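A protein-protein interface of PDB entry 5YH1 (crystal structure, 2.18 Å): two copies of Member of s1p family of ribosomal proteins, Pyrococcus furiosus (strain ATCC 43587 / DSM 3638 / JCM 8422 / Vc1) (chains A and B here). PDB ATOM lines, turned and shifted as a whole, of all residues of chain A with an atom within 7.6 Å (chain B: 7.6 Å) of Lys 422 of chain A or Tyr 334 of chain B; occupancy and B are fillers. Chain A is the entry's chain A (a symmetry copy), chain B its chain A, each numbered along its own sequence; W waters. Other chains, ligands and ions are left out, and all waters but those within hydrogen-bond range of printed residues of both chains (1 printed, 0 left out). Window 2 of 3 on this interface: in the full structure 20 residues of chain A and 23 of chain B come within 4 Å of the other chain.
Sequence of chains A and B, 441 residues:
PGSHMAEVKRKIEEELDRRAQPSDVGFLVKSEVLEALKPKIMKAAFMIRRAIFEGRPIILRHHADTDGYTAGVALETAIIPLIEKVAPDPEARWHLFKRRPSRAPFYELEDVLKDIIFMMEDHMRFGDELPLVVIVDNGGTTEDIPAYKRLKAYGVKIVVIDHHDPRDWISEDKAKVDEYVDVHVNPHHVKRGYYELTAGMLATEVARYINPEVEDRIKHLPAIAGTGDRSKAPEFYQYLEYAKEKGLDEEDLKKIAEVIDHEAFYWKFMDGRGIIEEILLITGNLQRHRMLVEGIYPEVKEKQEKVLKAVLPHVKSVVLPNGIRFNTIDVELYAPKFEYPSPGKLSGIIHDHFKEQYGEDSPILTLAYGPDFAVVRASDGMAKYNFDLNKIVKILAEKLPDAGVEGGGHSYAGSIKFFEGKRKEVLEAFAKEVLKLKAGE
Water W1 lies within hydrogen-bond range of O of Ala 335 of chain B (2.9 Å), N of Glu 420 of chain A (3.0 Å) and O of Glu 332 of chain B (3.1 Å).
Printed residues of chain B within 4 Å of Asp 402 of chain A: Ala 310 (3.5 Å) and His 314 (2.8 Å). Of the printed residues of chain B, Phe 419 of chain A touches Ala 310 (3.6 Å), Val 311 (3.9 Å), Leu 333 (3.4 Å), Tyr 334 (3.9 Å), Ala 335 (3.7 Å) and Pro 336 (3.8 Å). Lys 422 of chain A touches just one residue of chain B: Tyr 334 (3.9 Å). Printed residues of chain A within 4 Å of Val 311 of chain B: Phe 419. Of the printed residues of chain A, Leu 333 of chain B touches Phe 419, Glu 420 and Gly 421. Of the printed residues of chain A, Tyr 334 of chain B touches Phe 419 (3.9 Å), Gly 421 (3.8 Å) and Lys 422 (3.9 Å). Printed residues of chain A within 4 Å of Pro 336 of chain B: Phe 419 (3.8 Å). Lys 337 of chain B touches none of the printed residues of chain A. The nearest residue of chain A that does not touch Tyr 334 of chain B is Glu 420 of chain A (5.2 Å).
Asp 402 of chain A touches Ala 310 of chain B. Phe 419 of chain A touches Ala 310 of chain B. Phe 419 of chain A touches Val 311 of chain B (CZ to CG2, 3.9 Å). Leu 333 of chain B touches Phe 419 of chain A. Tyr 334 of chain B touches Phe 419 of chain A (CA to CG, 3.9 Å). Ala 335 of chain B touches Phe 419 of chain A (CA to CE1, 3.7 Å). Pro 336 of chain B touches Phe 419 of chain A (N to CE1, 3.8 Å). CA of Gly 421 of chain A touches CE1 of Tyr 334 of chain B (3.8 Å). CD of Lys 422 of chain A touches CE1 of Tyr 334 of chain B (3.9 Å).
No position is printed for both chains. Of the 12 pairs that touch across the chains among the printed residues, none has its exchanged pair printed and touching as well.
The backbone carbonyl oxygen (O) of Leu 333 of chain B sits at hydrogen-bond distance from the backbone NH (N) of Gly 421 of chain A (2.8 Å). The backbone carbonyl oxygen (O) of Leu 333 of chain B is in hydrogen-bond range of the backbone NH (N) of Glu 420 of chain A (3.2 Å). A ring nitrogen (NE2) of His 314 of chain B lies within hydrogen-bond range of the side-chain carboxylate of Asp 402 of chain A, at 3.2 Å.
NZ of Lys 422 of chain A lies within salt-bridge range of OD2 of Asp 402 of chain A, 2.9 Å away. The side-chain carboxylate (OD1) of Asp 330 of chain B is in hydrogen-bond range of the backbone NH (N) of Leu 333 of chain B (2.9 Å). The backbone NH (N) of Phe 419 of chain A is in hydrogen-bond range of the backbone carbonyl oxygen (O) of Ala 403 of chain A (2.8 Å).
Of the 18 printed residues of chain A, 5 touch a printed residue of chain B. Hydrophobic or aromatic side chains of chain A within 4 Å of the printed part of chain B: Phe 419. Among the printed residues, no Asp or Glu carboxylate lies within 4 Å of a Lys or Arg side-chain nitrogen of the other chain.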
ATOM      1  N   PRO A 371     -27.639  -5.895  -1.147  1.00  0.00           N
ATOM      2  CA  PRO A 371     -26.746  -7.045  -0.951  1.00  0.00           C
ATOM      3  C   PRO A 371     -27.200  -8.294  -1.707  1.00  0.00           C
ATOM      4  O   PRO A 371     -26.369  -9.002  -2.258  1.00  0.00           O
ATOM      5  CB  PRO A 371     -26.829  -7.319   0.566  1.00  0.00           C
ATOM      6  CG  PRO A 371     -27.417  -6.095   1.172  1.00  0.00           C
ATOM      7  CD  PRO A 371     -28.297  -5.489   0.110  1.00  0.00           C
ATOM      8  N   LEU A 400     -25.740 -19.697 -13.648  1.00  0.00           N
ATOM      9  CA  LEU A 400     -25.206 -19.551 -12.284  1.00  0.00           C
ATOM     10  C   LEU A 400     -26.099 -20.329 -11.331  1.00  0.00           C
ATOM     11  O   LEU A 400     -26.806 -19.736 -10.510  1.00  0.00           O
ATOM     12  CB  LEU A 400     -25.166 -18.070 -11.877  1.00  0.00           C
ATOM     13  CG  LEU A 400     -24.399 -17.132 -12.808  1.00  0.00           C
ATOM     14  CD1 LEU A 400     -24.662 -15.670 -12.457  1.00  0.00           C
ATOM     15  CD2 LEU A 400     -22.911 -17.428 -12.760  1.00  0.00           C
ATOM     16  N   PRO A 401     -26.085 -21.670 -11.447  1.00  0.00           N
ATOM     17  CA  PRO A 401     -27.015 -22.499 -10.665  1.00  0.00           C
ATOM     18  C   PRO A 401     -26.779 -22.439  -9.144  1.00  0.00           C
ATOM     19  O   PRO A 401     -27.708 -22.654  -8.363  1.00  0.00           O
ATOM     20  CB  PRO A 401     -26.788 -23.917 -11.227  1.00  0.00           C
ATOM     21  CG  PRO A 401     -25.442 -23.881 -11.890  1.00  0.00           C
ATOM     22  CD  PRO A 401     -25.209 -22.467 -12.330  1.00  0.00           C
ATOM     23  N   ASP A 402     -25.561 -22.100  -8.738  1.00  0.00           N
ATOM     24  CA  ASP A 402     -25.207 -21.950  -7.320  1.00  0.00           C
ATOM     25  C   ASP A 402     -25.465 -20.549  -6.733  1.00  0.00           C
ATOM     26  O   ASP A 402     -25.126 -20.296  -5.580  1.00  0.00           O
ATOM     27  CB  ASP A 402     -23.719 -22.279  -7.142  1.00  0.00           C
ATOM     28  CG  ASP A 402     -22.822 -21.285  -7.847  1.00  0.00           C
ATOM     29  OD1 ASP A 402     -23.244 -20.750  -8.913  1.00  0.00           O
ATOM     30  OD2 ASP A 402     -21.698 -21.035  -7.361  1.00  0.00           O
ATOM     31  N   ALA A 403     -26.042 -19.628  -7.502  1.00  0.00           N
ATOM     32  CA  ALA A 403     -26.200 -18.249  -7.021  1.00  0.00           C
ATOM     33  C   ALA A 403     -27.599 -17.939  -6.467  1.00  0.00           C
ATOM     34  O   ALA A 403     -27.868 -16.802  -6.077  1.00  0.00           O
ATOM     35  CB  ALA A 403     -25.840 -17.273  -8.121  1.00  0.00           C
ATOM     36  N   GLY A 404     -28.487 -18.930  -6.446  1.00  0.00           N
ATOM     37  CA  GLY A 404     -29.834 -18.756  -5.886  1.00  0.00           C
ATOM     38  C   GLY A 404     -30.678 -17.703  -6.593  1.00  0.00           C
ATOM     39  O   GLY A 404     -31.480 -17.020  -5.960  1.00  0.00           O
ATOM     40  N   VAL A 405     -30.512 -17.584  -7.907  1.00  0.00           N
ATOM     41  CA  VAL A 405     -31.212 -16.555  -8.676  1.00  0.00           C
ATOM     42  C   VAL A 405     -32.707 -16.850  -8.756  1.00  0.00           C
ATOM     43  O   VAL A 405     -33.109 -17.973  -9.023  1.00  0.00           O
ATOM     44  CB  VAL A 405     -30.647 -16.425 -10.100  1.00  0.00           C
ATOM     45  CG1 VAL A 405     -31.431 -15.384 -10.887  1.00  0.00           C
ATOM     46  CG2 VAL A 405     -29.165 -16.063 -10.059  1.00  0.00           C
ATOM     47  N   PHE A 418     -30.908 -13.103  -5.160  1.00  0.00           N
ATOM     48  CA  PHE A 418     -29.740 -13.956  -5.348  1.00  0.00           C
ATOM     49  C   PHE A 418     -28.968 -14.034  -4.025  1.00  0.00           C
ATOM     50  O   PHE A 418     -29.282 -13.298  -3.080  1.00  0.00           O
ATOM     51  CB  PHE A 418     -28.848 -13.389  -6.450  1.00  0.00           C
ATOM     52  CG  PHE A 418     -28.666 -11.895  -6.366  1.00  0.00           C
ATOM     53  CD1 PHE A 418     -27.700 -11.343  -5.539  1.00  0.00           C
ATOM     54  CD2 PHE A 418     -29.465 -11.041  -7.118  1.00  0.00           C
ATOM     55  CE1 PHE A 418     -27.543  -9.971  -5.455  1.00  0.00           C
ATOM     56  CE2 PHE A 418     -29.302  -9.669  -7.040  1.00  0.00           C
ATOM     57  CZ  PHE A 418     -28.343  -9.134  -6.212  1.00  0.00           C
ATOM     58  N   PHE A 419     -27.976 -14.919  -3.971  1.00  0.00           N
ATOM     59  CA  PHE A 419     -27.096 -15.039  -2.804  1.00  0.00           C
ATOM     60  C   PHE A 419     -26.136 -13.854  -2.750  1.00  0.00           C
ATOM     61  O   PHE A 419     -25.519 -13.502  -3.762  1.00  0.00           O
ATOM     62  CB  PHE A 419     -26.277 -16.338  -2.864  1.00  0.00           C
ATOM     63  CG  PHE A 419     -27.076 -17.600  -2.653  1.00  0.00           C
ATOM     64  CD1 PHE A 419     -28.330 -17.592  -2.052  1.00  0.00           C
ATOM     65  CD2 PHE A 419     -26.545 -18.819  -3.043  1.00  0.00           C
ATOM     66  CE1 PHE A 419     -29.039 -18.773  -1.874  1.00  0.00           C
ATOM     67  CE2 PHE A 419     -27.245 -19.999  -2.862  1.00  0.00           C
ATOM     68  CZ  PHE A 419     -28.491 -19.980  -2.273  1.00  0.00           C
ATOM     69  N   GLU A 420     -25.990 -13.251  -1.571  1.00  0.00           N
ATOM     70  CA  GLU A 420     -25.149 -12.062  -1.431  1.00  0.00           C
ATOM     71  C   GLU A 420     -23.722 -12.289  -1.910  1.00  0.00           C
ATOM     72  O   GLU A 420     -23.116 -11.412  -2.531  1.00  0.00           O
ATOM     73  CB  GLU A 420     -25.144 -11.574   0.020  1.00  0.00           C
ATOM     74  CG  GLU A 420     -24.163 -10.443   0.287  1.00  0.00           C
ATOM     75  CD  GLU A 420     -24.276  -9.881   1.693  1.00  0.00           C
ATOM     76  OE1 GLU A 420     -23.478  -8.976   2.015  1.00  0.00           O
ATOM     77  OE2 GLU A 420     -25.146 -10.334   2.471  1.00  0.00           O
ATOM     78  N   GLY A 421     -23.190 -13.477  -1.636  1.00  0.00           N
ATOM     79  CA  GLY A 421     -21.836 -13.817  -2.036  1.00  0.00           C
ATOM     80  C   GLY A 421     -21.639 -14.018  -3.526  1.00  0.00           C
ATOM     81  O   GLY A 421     -20.507 -14.145  -3.967  1.00  0.00           O
ATOM     82  N   LYS A 422     -22.722 -14.059  -4.306  1.00  0.00           N
ATOM     83  CA  LYS A 422     -22.615 -14.158  -5.763  1.00  0.00           C
ATOM     84  C   LYS A 422     -23.150 -12.900  -6.473  1.00  0.00           C
ATOM     85  O   LYS A 422     -23.437 -12.945  -7.670  1.00  0.00           O
ATOM     86  CB  LYS A 422     -23.363 -15.400  -6.275  1.00  0.00           C
ATOM     87  CG  LYS A 422     -22.860 -16.759  -5.779  1.00  0.00           C
ATOM     88  CD  LYS A 422     -21.346 -16.925  -5.815  1.00  0.00           C
ATOM     89  CE  LYS A 422     -20.766 -16.944  -7.216  1.00  0.00           C
ATOM     90  NZ  LYS A 422     -20.703 -18.332  -7.740  1.00  0.00           N
ATOM     91  N   ARG A 423     -23.272 -11.785  -5.750  1.00  0.00           N
ATOM     92  CA  ARG A 423     -23.843 -10.571  -6.331  1.00  0.00           C
ATOM     93  C   ARG A 423     -23.081 -10.086  -7.564  1.00  0.00           C
ATOM     94  O   ARG A 423     -23.678  -9.833  -8.606  1.00  0.00           O
ATOM     95  CB  ARG A 423     -23.906  -9.429  -5.322  1.00  0.00           C
ATOM     96  CG  ARG A 423     -24.515  -8.180  -5.951  1.00  0.00           C
ATOM     97  CD  ARG A 423     -24.754  -7.080  -4.945  1.00  0.00           C
ATOM     98  NE  ARG A 423     -23.502  -6.510  -4.487  1.00  0.00           N
ATOM     99  CZ  ARG A 423     -23.416  -5.511  -3.623  1.00  0.00           C
ATOM    100  NH1 ARG A 423     -22.227  -5.062  -3.247  1.00  0.00           N
ATOM    101  NH2 ARG A 423     -24.520  -4.967  -3.126  1.00  0.00           N
ATOM    102  N   LYS A 424     -21.771  -9.946  -7.422  1.00  0.00           N
ATOM    103  CA  LYS A 424     -20.909  -9.471  -8.501  1.00  0.00           C
ATOM    104  C   LYS A 424     -21.148 -10.293  -9.779  1.00  0.00           C
ATOM    105  O   LYS A 424     -21.373  -9.727 -10.849  1.00  0.00           O
ATOM    106  CB  LYS A 424     -19.452  -9.574  -8.064  1.00  0.00           C
ATOM    107  CG  LYS A 424     -18.431  -8.877  -8.948  1.00  0.00           C
ATOM    108  CD  LYS A 424     -17.059  -9.514  -8.741  1.00  0.00           C
ATOM    109  CE  LYS A 424     -15.915  -8.533  -8.928  1.00  0.00           C
ATOM    110  NZ  LYS A 424     -15.805  -8.055 -10.332  1.00  0.00           N
ATOM    111  N   GLU A 425     -21.120 -11.622  -9.652  1.00  0.00           N
ATOM    112  CA  GLU A 425     -21.287 -12.514 -10.796  1.00  0.00           C
ATOM    113  C   GLU A 425     -22.682 -12.397 -11.419  1.00  0.00           C
ATOM    114  O   GLU A 425     -22.820 -12.385 -12.637  1.00  0.00           O
ATOM    115  CB  GLU A 425     -21.020 -13.979 -10.410  1.00  0.00           C
ATOM    116  CG  GLU A 425     -19.566 -14.309 -10.097  1.00  0.00           C
ATOM    117  CD  GLU A 425     -19.182 -14.091  -8.635  1.00  0.00           C
ATOM    118  OE1 GLU A 425     -18.205 -14.723  -8.194  1.00  0.00           O
ATOM    119  OE2 GLU A 425     -19.836 -13.303  -7.911  1.00  0.00           O
ATOM    120  N   VAL A 426     -23.710 -12.327 -10.585  1.00  0.00           N
ATOM    121  CA  VAL A 426     -25.076 -12.208 -11.077  1.00  0.00           C
ATOM    122  C   VAL A 426     -25.300 -10.882 -11.832  1.00  0.00           C
ATOM    123  O   VAL A 426     -25.884 -10.870 -12.920  1.00  0.00           O
ATOM    124  CB  VAL A 426     -26.098 -12.353  -9.930  1.00  0.00           C
ATOM    125  CG1 VAL A 426     -27.503 -12.028 -10.408  1.00  0.00           C
ATOM    126  CG2 VAL A 426     -26.066 -13.768  -9.370  1.00  0.00           C
ATOM    127  N   LEU A 427     -24.824  -9.776 -11.267  1.00  0.00           N
ATOM    128  CA  LEU A 427     -25.066  -8.460 -11.865  1.00  0.00           C
ATOM    129  C   LEU A 427     -24.204  -8.218 -13.089  1.00  0.00           C
ATOM    130  O   LEU A 427     -24.648  -7.579 -14.029  1.00  0.00           O
ATOM    131  CB  LEU A 427     -24.856  -7.343 -10.844  1.00  0.00           C
ATOM    132  CG  LEU A 427     -25.840  -7.379  -9.673  1.00  0.00           C
ATOM    133  CD1 LEU A 427     -25.635  -6.153  -8.801  1.00  0.00           C
ATOM    134  CD2 LEU A 427     -27.287  -7.478 -10.145  1.00  0.00           C
ATOM    135  N   GLU A 428     -22.978  -8.726 -13.081  1.00  0.00           N
ATOM    136  CA  GLU A 428     -22.159  -8.694 -14.283  1.00  0.00           C
ATOM    137  C   GLU A 428     -22.765  -9.552 -15.395  1.00  0.00           C
ATOM    138  O   GLU A 428     -22.724  -9.163 -16.561  1.00  0.00           O
ATOM    139  CB  GLU A 428     -20.723  -9.106 -13.982  1.00  0.00           C
ATOM    140  CG  GLU A 428     -19.955  -8.022 -13.248  1.00  0.00           C
ATOM    141  CD  GLU A 428     -18.510  -8.389 -12.972  1.00  0.00           C
ATOM    142  OE1 GLU A 428     -18.118  -9.549 -13.233  1.00  0.00           O
ATOM    143  OE2 GLU A 428     -17.767  -7.508 -12.488  1.00  0.00           O
ATOM    144  N   VAL B 307     -33.051 -25.493  -1.927  1.00  0.00           N
ATOM    145  CA  VAL B 307     -32.070 -24.723  -1.156  1.00  0.00           C
ATOM    146  C   VAL B 307     -30.789 -25.550  -0.992  1.00  0.00           C
ATOM    147  O   VAL B 307     -29.687 -25.045  -1.170  1.00  0.00           O
ATOM    148  CB  VAL B 307     -32.648 -24.206   0.194  1.00  0.00           C
ATOM    149  CG1 VAL B 307     -32.834 -25.335   1.198  1.00  0.00           C
ATOM    150  CG2 VAL B 307     -31.747 -23.141   0.795  1.00  0.00           C
ATOM    151  N   ALA B 310     -28.671 -25.492  -4.197  1.00  0.00           N
ATOM    152  CA  ALA B 310     -28.024 -24.198  -4.423  1.00  0.00           C
ATOM    153  C   ALA B 310     -26.889 -23.900  -3.437  1.00  0.00           C
ATOM    154  O   ALA B 310     -25.921 -23.219  -3.797  1.00  0.00           O
ATOM    155  CB  ALA B 310     -29.060 -23.084  -4.375  1.00  0.00           C
ATOM    156  N   VAL B 311     -27.009 -24.398  -2.202  1.00  0.00           N
ATOM    157  CA  VAL B 311     -26.074 -24.052  -1.121  1.00  0.00           C
ATOM    158  C   VAL B 311     -24.877 -25.006  -1.017  1.00  0.00           C
ATOM    159  O   VAL B 311     -23.757 -24.592  -0.695  1.00  0.00           O
ATOM    160  CB  VAL B 311     -26.813 -23.989   0.241  1.00  0.00           C
ATOM    161  CG1 VAL B 311     -25.842 -23.744   1.383  1.00  0.00           C
ATOM    162  CG2 VAL B 311     -27.858 -22.882   0.218  1.00  0.00           C
ATOM    163  N   LEU B 312     -25.121 -26.278  -1.298  1.00  0.00           N
ATOM    164  CA  LEU B 312     -24.110 -27.340  -1.172  1.00  0.00           C
ATOM    165  C   LEU B 312     -22.778 -27.063  -1.866  1.00  0.00           C
ATOM    166  O   LEU B 312     -21.732 -27.349  -1.304  1.00  0.00           O
ATOM    167  CB  LEU B 312     -24.690 -28.656  -1.689  1.00  0.00           C
ATOM    168  CG  LEU B 312     -24.143 -29.963  -1.169  1.00  0.00           C
ATOM    169  CD1 LEU B 312     -24.119 -29.991   0.358  1.00  0.00           C
ATOM    170  CD2 LEU B 312     -25.015 -31.083  -1.733  1.00  0.00           C
ATOM    171  N   PRO B 313     -22.799 -26.492  -3.086  1.00  0.00           N
ATOM    172  CA  PRO B 313     -21.519 -26.149  -3.722  1.00  0.00           C
ATOM    173  C   PRO B 313     -20.646 -25.172  -2.933  1.00  0.00           C
ATOM    174  O   PRO B 313     -19.455 -25.069  -3.203  1.00  0.00           O
ATOM    175  CB  PRO B 313     -21.951 -25.508  -5.046  1.00  0.00           C
ATOM    176  CG  PRO B 313     -23.250 -26.136  -5.346  1.00  0.00           C
ATOM    177  CD  PRO B 313     -23.927 -26.271  -4.005  1.00  0.00           C
ATOM    178  N   HIS B 314     -21.227 -24.459  -1.974  1.00  0.00           N
ATOM    179  CA  HIS B 314     -20.465 -23.519  -1.154  1.00  0.00           C
ATOM    180  C   HIS B 314     -20.029 -24.094   0.183  1.00  0.00           C
ATOM    181  O   HIS B 314     -19.358 -23.425   0.949  1.00  0.00           O
ATOM    182  CB  HIS B 314     -21.301 -22.257  -0.948  1.00  0.00           C
ATOM    183  CG  HIS B 314     -21.693 -21.618  -2.237  1.00  0.00           C
ATOM    184  ND1 HIS B 314     -22.983 -21.645  -2.717  1.00  0.00           N
ATOM    185  CD2 HIS B 314     -20.948 -21.006  -3.186  1.00  0.00           C
ATOM    186  CE1 HIS B 314     -23.019 -21.043  -3.892  1.00  0.00           C
ATOM    187  NE2 HIS B 314     -21.799 -20.643  -4.198  1.00  0.00           N
ATOM    188  N   VAL B 315     -20.386 -25.339   0.466  1.00  0.00           N
ATOM    189  CA  VAL B 315     -19.954 -25.971   1.712  1.00  0.00           C
ATOM    190  C   VAL B 315     -18.539 -26.506   1.514  1.00  0.00           C
ATOM    191  O   VAL B 315     -18.315 -27.288   0.615  1.00  0.00           O
ATOM    192  CB  VAL B 315     -20.898 -27.124   2.116  1.00  0.00           C
ATOM    193  CG1 VAL B 315     -20.444 -27.771   3.420  1.00  0.00           C
ATOM    194  CG2 VAL B 315     -22.323 -26.615   2.244  1.00  0.00           C
ATOM    195  N   ILE B 329     -19.949 -23.542   6.267  1.00  0.00           N
ATOM    196  CA  ILE B 329     -20.793 -22.845   5.308  1.00  0.00           C
ATOM    197  C   ILE B 329     -21.164 -21.469   5.847  1.00  0.00           C
ATOM    198  O   ILE B 329     -21.636 -21.328   6.978  1.00  0.00           O
ATOM    199  CB  ILE B 329     -22.057 -23.668   4.950  1.00  0.00           C
ATOM    200  CG1 ILE B 329     -23.001 -22.886   4.033  1.00  0.00           C
ATOM    201  CG2 ILE B 329     -22.807 -24.114   6.194  1.00  0.00           C
ATOM    202  CD1 ILE B 329     -22.428 -22.612   2.663  1.00  0.00           C
ATOM    203  N   ASP B 330     -20.922 -20.462   5.022  1.00  0.00           N
ATOM    204  CA  ASP B 330     -21.296 -19.082   5.322  1.00  0.00           C
ATOM    205  C   ASP B 330     -22.745 -18.882   4.899  1.00  0.00           C
ATOM    206  O   ASP B 330     -23.029 -18.648   3.716  1.00  0.00           O
ATOM    207  CB  ASP B 330     -20.373 -18.132   4.562  1.00  0.00           C
ATOM    208  CG  ASP B 330     -20.618 -16.665   4.903  1.00  0.00           C
ATOM    209  OD1 ASP B 330     -21.772 -16.300   5.251  1.00  0.00           O
ATOM    210  OD2 ASP B 330     -19.644 -15.887   4.806  1.00  0.00           O
ATOM    211  N   VAL B 331     -23.656 -18.982   5.861  1.00  0.00           N
ATOM    212  CA  VAL B 331     -25.076 -18.852   5.575  1.00  0.00           C
ATOM    213  C   VAL B 331     -25.572 -17.400   5.488  1.00  0.00           C
ATOM    214  O   VAL B 331     -26.742 -17.186   5.240  1.00  0.00           O
ATOM    215  CB  VAL B 331     -25.961 -19.662   6.549  1.00  0.00           C
ATOM    216  CG1 VAL B 331     -25.613 -21.142   6.463  1.00  0.00           C
ATOM    217  CG2 VAL B 331     -25.832 -19.165   7.984  1.00  0.00           C
ATOM    218  N   GLU B 332     -24.701 -16.417   5.682  1.00  0.00           N
ATOM    219  CA  GLU B 332     -25.045 -15.040   5.329  1.00  0.00           C
ATOM    220  C   GLU B 332     -24.819 -14.824   3.826  1.00  0.00           C
ATOM    221  O   GLU B 332     -25.687 -14.300   3.151  1.00  0.00           O
ATOM    222  CB  GLU B 332     -24.221 -14.033   6.137  1.00  0.00           C
ATOM    223  CG  GLU B 332     -24.771 -12.601   6.154  1.00  0.00           C
ATOM    224  CD  GLU B 332     -26.102 -12.422   6.915  1.00  0.00           C
ATOM    225  OE1 GLU B 332     -26.690 -11.326   6.791  1.00  0.00           O
ATOM    226  OE2 GLU B 332     -26.569 -13.341   7.638  1.00  0.00           O
ATOM    227  N   LEU B 333     -23.657 -15.229   3.310  1.00  0.00           N
ATOM    228  CA  LEU B 333     -23.338 -15.035   1.893  1.00  0.00           C
ATOM    229  C   LEU B 333     -24.063 -15.990   0.942  1.00  0.00           C
ATOM    230  O   LEU B 333     -24.387 -15.606  -0.190  1.00  0.00           O
ATOM    231  CB  LEU B 333     -21.834 -15.158   1.648  1.00  0.00           C
ATOM    232  CG  LEU B 333     -20.910 -14.098   2.247  1.00  0.00           C
ATOM    233  CD1 LEU B 333     -19.500 -14.294   1.708  1.00  0.00           C
ATOM    234  CD2 LEU B 333     -21.406 -12.686   1.954  1.00  0.00           C
ATOM    235  N   TYR B 334     -24.310 -17.226   1.381  1.00  0.00           N
ATOM    236  CA  TYR B 334     -24.771 -18.282   0.475  1.00  0.00           C
ATOM    237  C   TYR B 334     -26.026 -18.968   0.975  1.00  0.00           C
ATOM    238  O   TYR B 334     -26.113 -20.186   0.971  1.00  0.00           O
ATOM    239  CB  TYR B 334     -23.663 -19.323   0.269  1.00  0.00           C
ATOM    240  CG  TYR B 334     -22.375 -18.722  -0.230  1.00  0.00           C
ATOM    241  CD1 TYR B 334     -22.306 -18.140  -1.492  1.00  0.00           C
ATOM    242  CD2 TYR B 334     -21.229 -18.726   0.553  1.00  0.00           C
ATOM    243  CE1 TYR B 334     -21.126 -17.577  -1.958  1.00  0.00           C
ATOM    244  CE2 TYR B 334     -20.048 -18.166   0.096  1.00  0.00           C
ATOM    245  CZ  TYR B 334     -20.007 -17.592  -1.162  1.00  0.00           C
ATOM    246  OH  TYR B 334     -18.843 -17.033  -1.616  1.00  0.00           O
ATOM    247  N   ALA B 335     -26.992 -18.185   1.424  1.00  0.00           N
ATOM    248  CA  ALA B 335     -28.290 -18.720   1.791  1.00  0.00           C
ATOM    249  C   ALA B 335     -29.294 -17.593   1.667  1.00  0.00           C
ATOM    250  O   ALA B 335     -28.907 -16.439   1.740  1.00  0.00           O
ATOM    251  CB  ALA B 335     -28.264 -19.258   3.218  1.00  0.00           C
ATOM    252  N   PRO B 336     -30.584 -17.919   1.471  1.00  0.00           N
ATOM    253  CA  PRO B 336     -31.592 -16.869   1.339  1.00  0.00           C
ATOM    254  C   PRO B 336     -31.967 -16.288   2.693  1.00  0.00           C
ATOM    255  O   PRO B 336     -32.541 -16.990   3.523  1.00  0.00           O
ATOM    256  CB  PRO B 336     -32.784 -17.605   0.713  1.00  0.00           C
ATOM    257  CG  PRO B 336     -32.642 -19.016   1.166  1.00  0.00           C
ATOM    258  CD  PRO B 336     -31.166 -19.269   1.334  1.00  0.00           C
ATOM    259  N   LYS B 337     -31.652 -15.018   2.921  1.00  0.00           N
ATOM    260  CA  LYS B 337     -31.932 -14.410   4.213  1.00  0.00           C
ATOM    261  C   LYS B 337     -33.438 -14.203   4.415  1.00  0.00           C
ATOM    262  O   LYS B 337     -34.167 -13.891   3.464  1.00  0.00           O
ATOM    263  CB  LYS B 337     -31.177 -13.091   4.377  1.00  0.00           C
ATOM    264  CG  LYS B 337     -31.082 -12.664   5.833  1.00  0.00           C
ATOM    265  CD  LYS B 337     -30.198 -11.441   6.023  1.00  0.00           C
ATOM    266  CE  LYS B 337     -29.954 -11.173   7.501  1.00  0.00           C
ATOM    267  NZ  LYS B 337     -29.121  -9.958   7.705  1.00  0.00           N
ATOM    268  N   LEU B 346     -31.449 -24.872   8.123  1.00  0.00           N
ATOM    269  CA  LEU B 346     -30.555 -25.070   6.986  1.00  0.00           C
ATOM    270  C   LEU B 346     -29.327 -25.881   7.368  1.00  0.00           C
ATOM    271  O   LEU B 346     -28.931 -26.784   6.638  1.00  0.00           O
ATOM    272  CB  LEU B 346     -30.111 -23.728   6.393  1.00  0.00           C
ATOM    273  CG  LEU B 346     -29.140 -23.787   5.209  1.00  0.00           C
ATOM    274  CD1 LEU B 346     -29.702 -24.631   4.066  1.00  0.00           C
ATOM    275  CD2 LEU B 346     -28.834 -22.386   4.720  1.00  0.00           C
ATOM    276  N   ILE B 350     -28.119 -29.487   5.719  1.00  0.00           N
ATOM    277  CA  ILE B 350     -26.772 -29.732   5.207  1.00  0.00           C
ATOM    278  C   ILE B 350     -26.123 -30.874   5.990  1.00  0.00           C
ATOM    279  O   ILE B 350     -25.541 -31.802   5.403  1.00  0.00           O
ATOM    280  CB  ILE B 350     -25.913 -28.459   5.271  1.00  0.00           C
ATOM    281  CG1 ILE B 350     -26.440 -27.421   4.262  1.00  0.00           C
ATOM    282  CG2 ILE B 350     -24.446 -28.766   4.981  1.00  0.00           C
ATOM    283  CD1 ILE B 350     -26.007 -25.994   4.555  1.00  0.00           C
ATOM    284  N   TYR B 369     -22.166 -20.499   9.734  1.00  0.00           N
ATOM    285  CA  TYR B 369     -21.946 -19.203  10.381  1.00  0.00           C
ATOM    286  C   TYR B 369     -22.504 -18.005   9.609  1.00  0.00           C
ATOM    287  O   TYR B 369     -22.579 -18.003   8.378  1.00  0.00           O
ATOM    288  CB  TYR B 369     -20.460 -18.993  10.664  1.00  0.00           C
ATOM    289  CG  TYR B 369     -19.568 -18.987   9.448  1.00  0.00           C
ATOM    290  CD1 TYR B 369     -19.307 -17.804   8.751  1.00  0.00           C
ATOM    291  CD2 TYR B 369     -18.969 -20.160   8.997  1.00  0.00           C
ATOM    292  CE1 TYR B 369     -18.481 -17.803   7.635  1.00  0.00           C
ATOM    293  CE2 TYR B 369     -18.142 -20.168   7.884  1.00  0.00           C
ATOM    294  CZ  TYR B 369     -17.904 -18.992   7.209  1.00  0.00           C
ATOM    295  OH  TYR B 369     -17.084 -19.007   6.110  1.00  0.00           O
HETATM  296  O   HOH W   1     -27.694 -14.012   0.777  1.00  0.00           O
